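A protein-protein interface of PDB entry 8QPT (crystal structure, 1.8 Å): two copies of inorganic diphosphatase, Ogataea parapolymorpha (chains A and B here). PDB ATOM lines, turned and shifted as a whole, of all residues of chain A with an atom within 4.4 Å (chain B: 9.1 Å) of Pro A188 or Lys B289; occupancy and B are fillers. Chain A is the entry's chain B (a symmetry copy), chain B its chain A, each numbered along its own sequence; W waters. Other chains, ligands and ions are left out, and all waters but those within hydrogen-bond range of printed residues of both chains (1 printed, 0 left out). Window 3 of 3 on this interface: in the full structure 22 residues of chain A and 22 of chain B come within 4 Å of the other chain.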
ATOM      1  N   VAL A 183      -7.476   9.796  11.837  1.00  0.00           N
ATOM      2  CA  VAL A 183      -8.942  10.122  11.923  1.00  0.00           C
ATOM      3  C   VAL A 183      -9.656   9.234  10.899  1.00  0.00           C
ATOM      4  O   VAL A 183     -10.652   8.617  11.289  1.00  0.00           O
ATOM      5  CB  VAL A 183      -9.243  11.593  11.691  1.00  0.00           C
ATOM      6  CG1 VAL A 183     -10.755  11.820  11.765  1.00  0.00           C
ATOM      7  CG2 VAL A 183      -8.449  12.465  12.628  1.00  0.00           C
ATOM      8  N   TYR A 184      -9.122   9.190   9.681  1.00  0.00           N
ATOM      9  CA  TYR A 184      -9.669   8.373   8.576  1.00  0.00           C
ATOM     10  C   TYR A 184      -9.829   6.922   9.035  1.00  0.00           C
ATOM     11  O   TYR A 184     -10.913   6.334   8.876  1.00  0.00           O
ATOM     12  CB  TYR A 184      -8.803   8.579   7.325  1.00  0.00           C
ATOM     13  CG  TYR A 184      -9.148   7.670   6.174  1.00  0.00           C
ATOM     14  CD1 TYR A 184     -10.285   7.835   5.407  1.00  0.00           C
ATOM     15  CD2 TYR A 184      -8.344   6.573   5.902  1.00  0.00           C
ATOM     16  CE1 TYR A 184     -10.587   6.968   4.367  1.00  0.00           C
ATOM     17  CE2 TYR A 184      -8.612   5.705   4.847  1.00  0.00           C
ATOM     18  CZ  TYR A 184      -9.737   5.913   4.067  1.00  0.00           C
ATOM     19  OH  TYR A 184     -10.028   5.098   3.004  1.00  0.00           O
ATOM     20  N   GLU A 185      -8.855   6.381   9.745  1.00  0.00           N
ATOM     21  CA  GLU A 185      -8.913   4.953  10.172  1.00  0.00           C
ATOM     22  C   GLU A 185      -9.673   4.767  11.472  1.00  0.00           C
ATOM     23  O   GLU A 185     -10.430   3.769  11.577  1.00  0.00           O
ATOM     24  CB  GLU A 185      -7.478   4.384  10.208  1.00  0.00           C
ATOM     25  CG  GLU A 185      -6.777   4.608   8.838  1.00  0.00           C
ATOM     26  CD  GLU A 185      -5.462   3.861   8.595  1.00  0.00           C
ATOM     27  OE1 GLU A 185      -4.747   3.548   9.600  1.00  0.00           O
ATOM     28  OE2 GLU A 185      -5.102   3.691   7.391  1.00  0.00           O
ATOM     29  N   LYS A 186      -9.541   5.650  12.465  1.00  0.00           N
ATOM     30  CA  LYS A 186     -10.090   5.343  13.805  1.00  0.00           C
ATOM     31  C   LYS A 186     -11.428   6.058  14.088  1.00  0.00           C
ATOM     32  O   LYS A 186     -11.999   5.777  15.110  1.00  0.00           O
ATOM     33  CB  LYS A 186      -9.063   5.662  14.859  1.00  0.00           C
ATOM     34  CG  LYS A 186      -7.762   4.881  14.656  1.00  0.00           C
ATOM     35  CD  LYS A 186      -6.769   5.192  15.723  1.00  0.00           C
ATOM     36  CE  LYS A 186      -5.338   4.932  15.298  1.00  0.00           C
ATOM     37  NZ  LYS A 186      -4.531   4.953  16.536  1.00  0.00           N
ATOM     38  N   MET A 187     -11.804   6.983  13.224  1.00  0.00           N
ATOM     39  CA  MET A 187     -13.082   7.772  13.383  1.00  0.00           C
ATOM     40  C   MET A 187     -13.763   7.749  12.048  1.00  0.00           C
ATOM     41  O   MET A 187     -13.849   8.743  11.331  1.00  0.00           O
ATOM     42  CB  MET A 187     -12.761   9.173  13.864  1.00  0.00           C
ATOM     43  CG  MET A 187     -12.344   9.215  15.327  1.00  0.00           C
ATOM     44  SD  MET A 187     -11.710  10.872  15.854  1.00  0.00           S
ATOM     45  CE  MET A 187     -13.272  11.719  16.165  1.00  0.00           C
ATOM     46  N   PRO A 188     -14.137   6.518  11.593  1.00  0.00           N
ATOM     47  CA  PRO A 188     -14.648   6.345  10.252  1.00  0.00           C
ATOM     48  C   PRO A 188     -15.814   7.321   9.998  1.00  0.00           C
ATOM     49  O   PRO A 188     -16.703   7.432  10.902  1.00  0.00           O
ATOM     50  CB  PRO A 188     -15.113   4.876  10.186  1.00  0.00           C
ATOM     51  CG  PRO A 188     -15.061   4.381  11.582  1.00  0.00           C
ATOM     52  CD  PRO A 188     -14.048   5.238  12.319  1.00  0.00           C
ATOM     53  N   GLY A 189     -15.750   7.952   8.838  1.00  0.00           N
ATOM     54  CA  GLY A 189     -16.811   8.793   8.296  1.00  0.00           C
ATOM     55  C   GLY A 189     -16.615  10.261   8.646  1.00  0.00           C
ATOM     56  O   GLY A 189     -17.196  11.091   7.952  1.00  0.00           O
ATOM     57  N   VAL A 190     -15.738  10.617   9.588  1.00  0.00           N
ATOM     58  CA  VAL A 190     -15.537  12.027  10.024  1.00  0.00           C
ATOM     59  C   VAL A 190     -14.968  12.899   8.920  1.00  0.00           C
ATOM     60  O   VAL A 190     -15.552  13.946   8.500  1.00  0.00           O
ATOM     61  CB  VAL A 190     -14.682  12.098  11.296  1.00  0.00           C
ATOM     62  CG1 VAL A 190     -14.308  13.550  11.575  1.00  0.00           C
ATOM     63  CG2 VAL A 190     -15.423  11.504  12.461  1.00  0.00           C
ATOM     64  N   ILE B  90     -25.367   7.978  15.860  1.00  0.00           N
ATOM     65  CA  ILE B  90     -24.735   7.172  14.790  1.00  0.00           C
ATOM     66  C   ILE B  90     -24.203   8.151  13.776  1.00  0.00           C
ATOM     67  O   ILE B  90     -25.015   8.706  12.967  1.00  0.00           O
ATOM     68  CB  ILE B  90     -25.771   6.209  14.222  1.00  0.00           C
ATOM     69  CG1 ILE B  90     -26.434   5.316  15.270  1.00  0.00           C
ATOM     70  CG2 ILE B  90     -25.154   5.483  13.037  1.00  0.00           C
ATOM     71  CD1 ILE B  90     -25.433   4.605  16.174  1.00  0.00           C
ATOM     72  N   TYR B  91     -22.927   8.459  13.873  1.00  0.00           N
ATOM     73  CA  TYR B  91     -22.323   9.624  13.222  1.00  0.00           C
ATOM     74  C   TYR B  91     -22.678   9.567  11.766  1.00  0.00           C
ATOM     75  O   TYR B  91     -22.579   8.505  11.188  1.00  0.00           O
ATOM     76  CB  TYR B  91     -20.800   9.640  13.371  1.00  0.00           C
ATOM     77  CG  TYR B  91     -20.149  10.821  12.699  1.00  0.00           C
ATOM     78  CD1 TYR B  91     -20.010  11.995  13.431  1.00  0.00           C
ATOM     79  CD2 TYR B  91     -19.712  10.801  11.389  1.00  0.00           C
ATOM     80  CE1 TYR B  91     -19.478  13.144  12.872  1.00  0.00           C
ATOM     81  CE2 TYR B  91     -19.144  11.927  10.820  1.00  0.00           C
ATOM     82  CZ  TYR B  91     -19.037  13.114  11.569  1.00  0.00           C
ATOM     83  OH  TYR B  91     -18.411  14.160  11.002  1.00  0.00           O
ATOM     84  N   PRO B  92     -23.113  10.668  11.113  1.00  0.00           N
ATOM     85  CA  PRO B  92     -23.190  12.010  11.707  1.00  0.00           C
ATOM     86  C   PRO B  92     -24.593  12.401  12.181  1.00  0.00           C
ATOM     87  O   PRO B  92     -24.836  13.566  12.410  1.00  0.00           O
ATOM     88  CB  PRO B  92     -22.759  12.897  10.508  1.00  0.00           C
ATOM     89  CG  PRO B  92     -23.253  12.143   9.272  1.00  0.00           C
ATOM     90  CD  PRO B  92     -23.301  10.667   9.669  1.00  0.00           C
ATOM     91  N   ARG B 196     -29.246   2.373   7.084  1.00  0.00           N
ATOM     92  CA  ARG B 196     -28.003   2.161   7.787  1.00  0.00           C
ATOM     93  C   ARG B 196     -28.241   2.340   9.278  1.00  0.00           C
ATOM     94  O   ARG B 196     -27.793   1.509  10.092  1.00  0.00           O
ATOM     95  CB  ARG B 196     -26.985   3.172   7.301  1.00  0.00           C
ATOM     96  CG  ARG B 196     -25.780   3.210   8.206  1.00  0.00           C
ATOM     97  CD  ARG B 196     -24.649   4.054   7.659  1.00  0.00           C
ATOM     98  NE  ARG B 196     -23.452   3.289   8.000  1.00  0.00           N
ATOM     99  CZ  ARG B 196     -22.617   3.591   8.968  1.00  0.00           C
ATOM    100  NH1 ARG B 196     -22.824   4.666   9.719  1.00  0.00           N
ATOM    101  NH2 ARG B 196     -21.570   2.805   9.159  1.00  0.00           N
ATOM    102  N   GLU B 199     -29.826  -0.676  10.713  1.00  0.00           N
ATOM    103  CA  GLU B 199     -28.828  -1.796  10.741  1.00  0.00           C
ATOM    104  C   GLU B 199     -27.880  -1.725  11.967  1.00  0.00           C
ATOM    105  O   GLU B 199     -27.639  -2.764  12.630  1.00  0.00           O
ATOM    106  CB  GLU B 199     -28.035  -1.760   9.450  1.00  0.00           C
ATOM    107  CG  GLU B 199     -27.029  -2.918   9.365  1.00  0.00           C
ATOM    108  CD  GLU B 199     -26.380  -3.086   7.980  1.00  0.00           C
ATOM    109  OE1 GLU B 199     -26.703  -2.332   6.992  1.00  0.00           O
ATOM    110  OE2 GLU B 199     -25.528  -3.917   7.903  1.00  0.00           O
ATOM    111  N   VAL B 200     -27.345  -0.535  12.313  1.00  0.00           N
ATOM    112  CA  VAL B 200     -26.161  -0.386  13.192  1.00  0.00           C
ATOM    113  C   VAL B 200     -26.478   0.239  14.523  1.00  0.00           C
ATOM    114  O   VAL B 200     -25.570   0.352  15.301  1.00  0.00           O
ATOM    115  CB  VAL B 200     -25.073   0.423  12.479  1.00  0.00           C
ATOM    116  CG1 VAL B 200     -24.734  -0.135  11.138  1.00  0.00           C
ATOM    117  CG2 VAL B 200     -25.463   1.921  12.244  1.00  0.00           C
ATOM    118  N   ILE B 203     -25.168  -1.306  17.757  1.00  0.00           N
ATOM    119  CA  ILE B 203     -23.737  -1.748  17.799  1.00  0.00           C
ATOM    120  C   ILE B 203     -22.997  -1.084  18.943  1.00  0.00           C
ATOM    121  O   ILE B 203     -22.229  -1.734  19.681  1.00  0.00           O
ATOM    122  CB  ILE B 203     -23.069  -1.528  16.463  1.00  0.00           C
ATOM    123  CG1 ILE B 203     -23.647  -2.514  15.441  1.00  0.00           C
ATOM    124  CG2 ILE B 203     -21.550  -1.611  16.593  1.00  0.00           C
ATOM    125  CD1 ILE B 203     -23.110  -2.414  14.073  1.00  0.00           C
ATOM    126  N   PRO B 209     -24.969  -6.143  14.231  1.00  0.00           N
ATOM    127  CA  PRO B 209     -25.771  -5.452  13.220  1.00  0.00           C
ATOM    128  C   PRO B 209     -27.093  -6.204  13.019  1.00  0.00           C
ATOM    129  O   PRO B 209     -27.174  -7.390  13.155  1.00  0.00           O
ATOM    130  CB  PRO B 209     -24.970  -5.480  11.939  1.00  0.00           C
ATOM    131  CG  PRO B 209     -23.677  -6.258  12.273  1.00  0.00           C
ATOM    132  CD  PRO B 209     -23.636  -6.544  13.757  1.00  0.00           C
ATOM    133  N   MET B 285     -20.363  10.736  20.179  1.00  0.00           N
ATOM    134  CA  MET B 285     -20.658  10.218  18.844  1.00  0.00           C
ATOM    135  C   MET B 285     -20.153   8.777  18.724  1.00  0.00           C
ATOM    136  O   MET B 285     -19.034   8.520  19.268  1.00  0.00           O
ATOM    137  CB  MET B 285     -19.982  11.100  17.810  1.00  0.00           C
ATOM    138  CG  MET B 285     -20.670  12.559  17.794  1.00  0.00           C
ATOM    139  SD  MET B 285     -19.803  13.734  16.758  1.00  0.00           S
ATOM    140  CE  MET B 285     -18.430  14.116  17.834  1.00  0.00           C
ATOM    141  N   SER B 286     -20.854   7.991  17.950  1.00  0.00           N
ATOM    142  CA  SER B 286     -20.463   6.589  17.573  1.00  0.00           C
ATOM    143  C   SER B 286     -20.068   6.537  16.118  1.00  0.00           C
ATOM    144  O   SER B 286     -20.848   6.961  15.253  1.00  0.00           O
ATOM    145  CB  SER B 286     -21.583   5.622  17.877  1.00  0.00           C
ATOM    146  OG  SER B 286     -22.001   5.720  19.233  1.00  0.00           O
ATOM    147  N   PHE B 287     -18.843   6.096  15.844  1.00  0.00           N
ATOM    148  CA  PHE B 287     -18.329   6.133  14.470  1.00  0.00           C
ATOM    149  C   PHE B 287     -18.260   4.702  13.996  1.00  0.00           C
ATOM    150  O   PHE B 287     -17.351   3.959  14.504  1.00  0.00           O
ATOM    151  CB  PHE B 287     -16.937   6.762  14.427  1.00  0.00           C
ATOM    152  CG  PHE B 287     -16.849   8.093  15.103  1.00  0.00           C
ATOM    153  CD1 PHE B 287     -17.336   9.225  14.439  1.00  0.00           C
ATOM    154  CD2 PHE B 287     -16.332   8.228  16.396  1.00  0.00           C
ATOM    155  CE1 PHE B 287     -17.321  10.463  15.048  1.00  0.00           C
ATOM    156  CE2 PHE B 287     -16.281   9.491  16.997  1.00  0.00           C
ATOM    157  CZ  PHE B 287     -16.827  10.600  16.326  1.00  0.00           C
ATOM    158  N   ILE B 288     -19.199   4.295  13.179  1.00  0.00           N
ATOM    159  CA  ILE B 288     -19.364   2.857  12.864  1.00  0.00           C
ATOM    160  C   ILE B 288     -18.831   2.641  11.455  1.00  0.00           C
ATOM    161  O   ILE B 288     -19.248   3.390  10.571  1.00  0.00           O
ATOM    162  CB  ILE B 288     -20.825   2.423  13.041  1.00  0.00           C
ATOM    163  CG1 ILE B 288     -21.145   2.371  14.525  1.00  0.00           C
ATOM    164  CG2 ILE B 288     -21.124   1.104  12.341  1.00  0.00           C
ATOM    165  CD1 ILE B 288     -22.545   2.596  14.772  1.00  0.00           C
ATOM    166  N   LYS B 289     -17.888   1.692  11.310  1.00  0.00           N
ATOM    167  CA  LYS B 289     -17.144   1.332  10.079  1.00  0.00           C
ATOM    168  C   LYS B 289     -18.146   1.269   8.939  1.00  0.00           C
ATOM    169  O   LYS B 289     -18.079   1.908   7.875  1.00  0.00           O
ATOM    170  CB  LYS B 289     -16.400   0.000  10.304  1.00  0.00           C
ATOM    171  OXT LYS B 289     -19.070   0.535   9.175  1.00  0.00           O
HETATM  172  O   HOH W   1     -19.315   6.776  10.415  1.00  0.00           O
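The backbone carbonyl oxygen (O) of Ser B286 is in hydrogen-bond range of the backbone NH (N) of Tyr B91 (2.9 Å).
The guanidinium group (NH2) of Arg B196 is in salt-bridge range of the chain-end carboxylate (OXT) of Lys B289, 3.4 Å away.
Among the printed residues, pairs that only touch across the chains: Met A187 with Phe B287, Pro A188 with Phe B287, Pro A188 with Lys B289, Gly A189 with Tyr B91, Val A190 with Tyr B91 and Val A190 with Phe B287.
Of the printed residues of chain B, Met A187 touches Phe B287 (3.7 Å).
Pro A188 touches just these residues of chain B: Phe B287 and Lys B289.
Of chain B, only Tyr B91 comes within 4 Å of Gly A189.
Printed residues of chain B within 4 Å of Val A190: Tyr B91 and Phe B287.
Met B285 touches none of the printed residues of chain A.
Lys B289 touches just one residue of chain A: Pro A188.
The nearest residue of chain B that does not touch Pro A188 is Ile B288 (4.2 Å).
The nearest printed residue of chain A that does not touch Tyr B91 is Pro A188 (4.5 Å).
Printed residues of chain A that touch a printed residue of chain B: Met A187, Pro A188, Gly A189 and Val A190.
Hydrophobic or aromatic side chains of chain A within 4 Å of the printed part of chain B: Met A187, Pro A188 and Val A190.
Among the printed residues, no Asp or Glu carboxylate lies within 4 Å of a Lys or Arg side-chain nitrogen of the other chain.
No position is printed for both chains.
Water W1 bridges O of Pro A188 (2.7 Å) and O of Ile B288 (3.4 Å).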
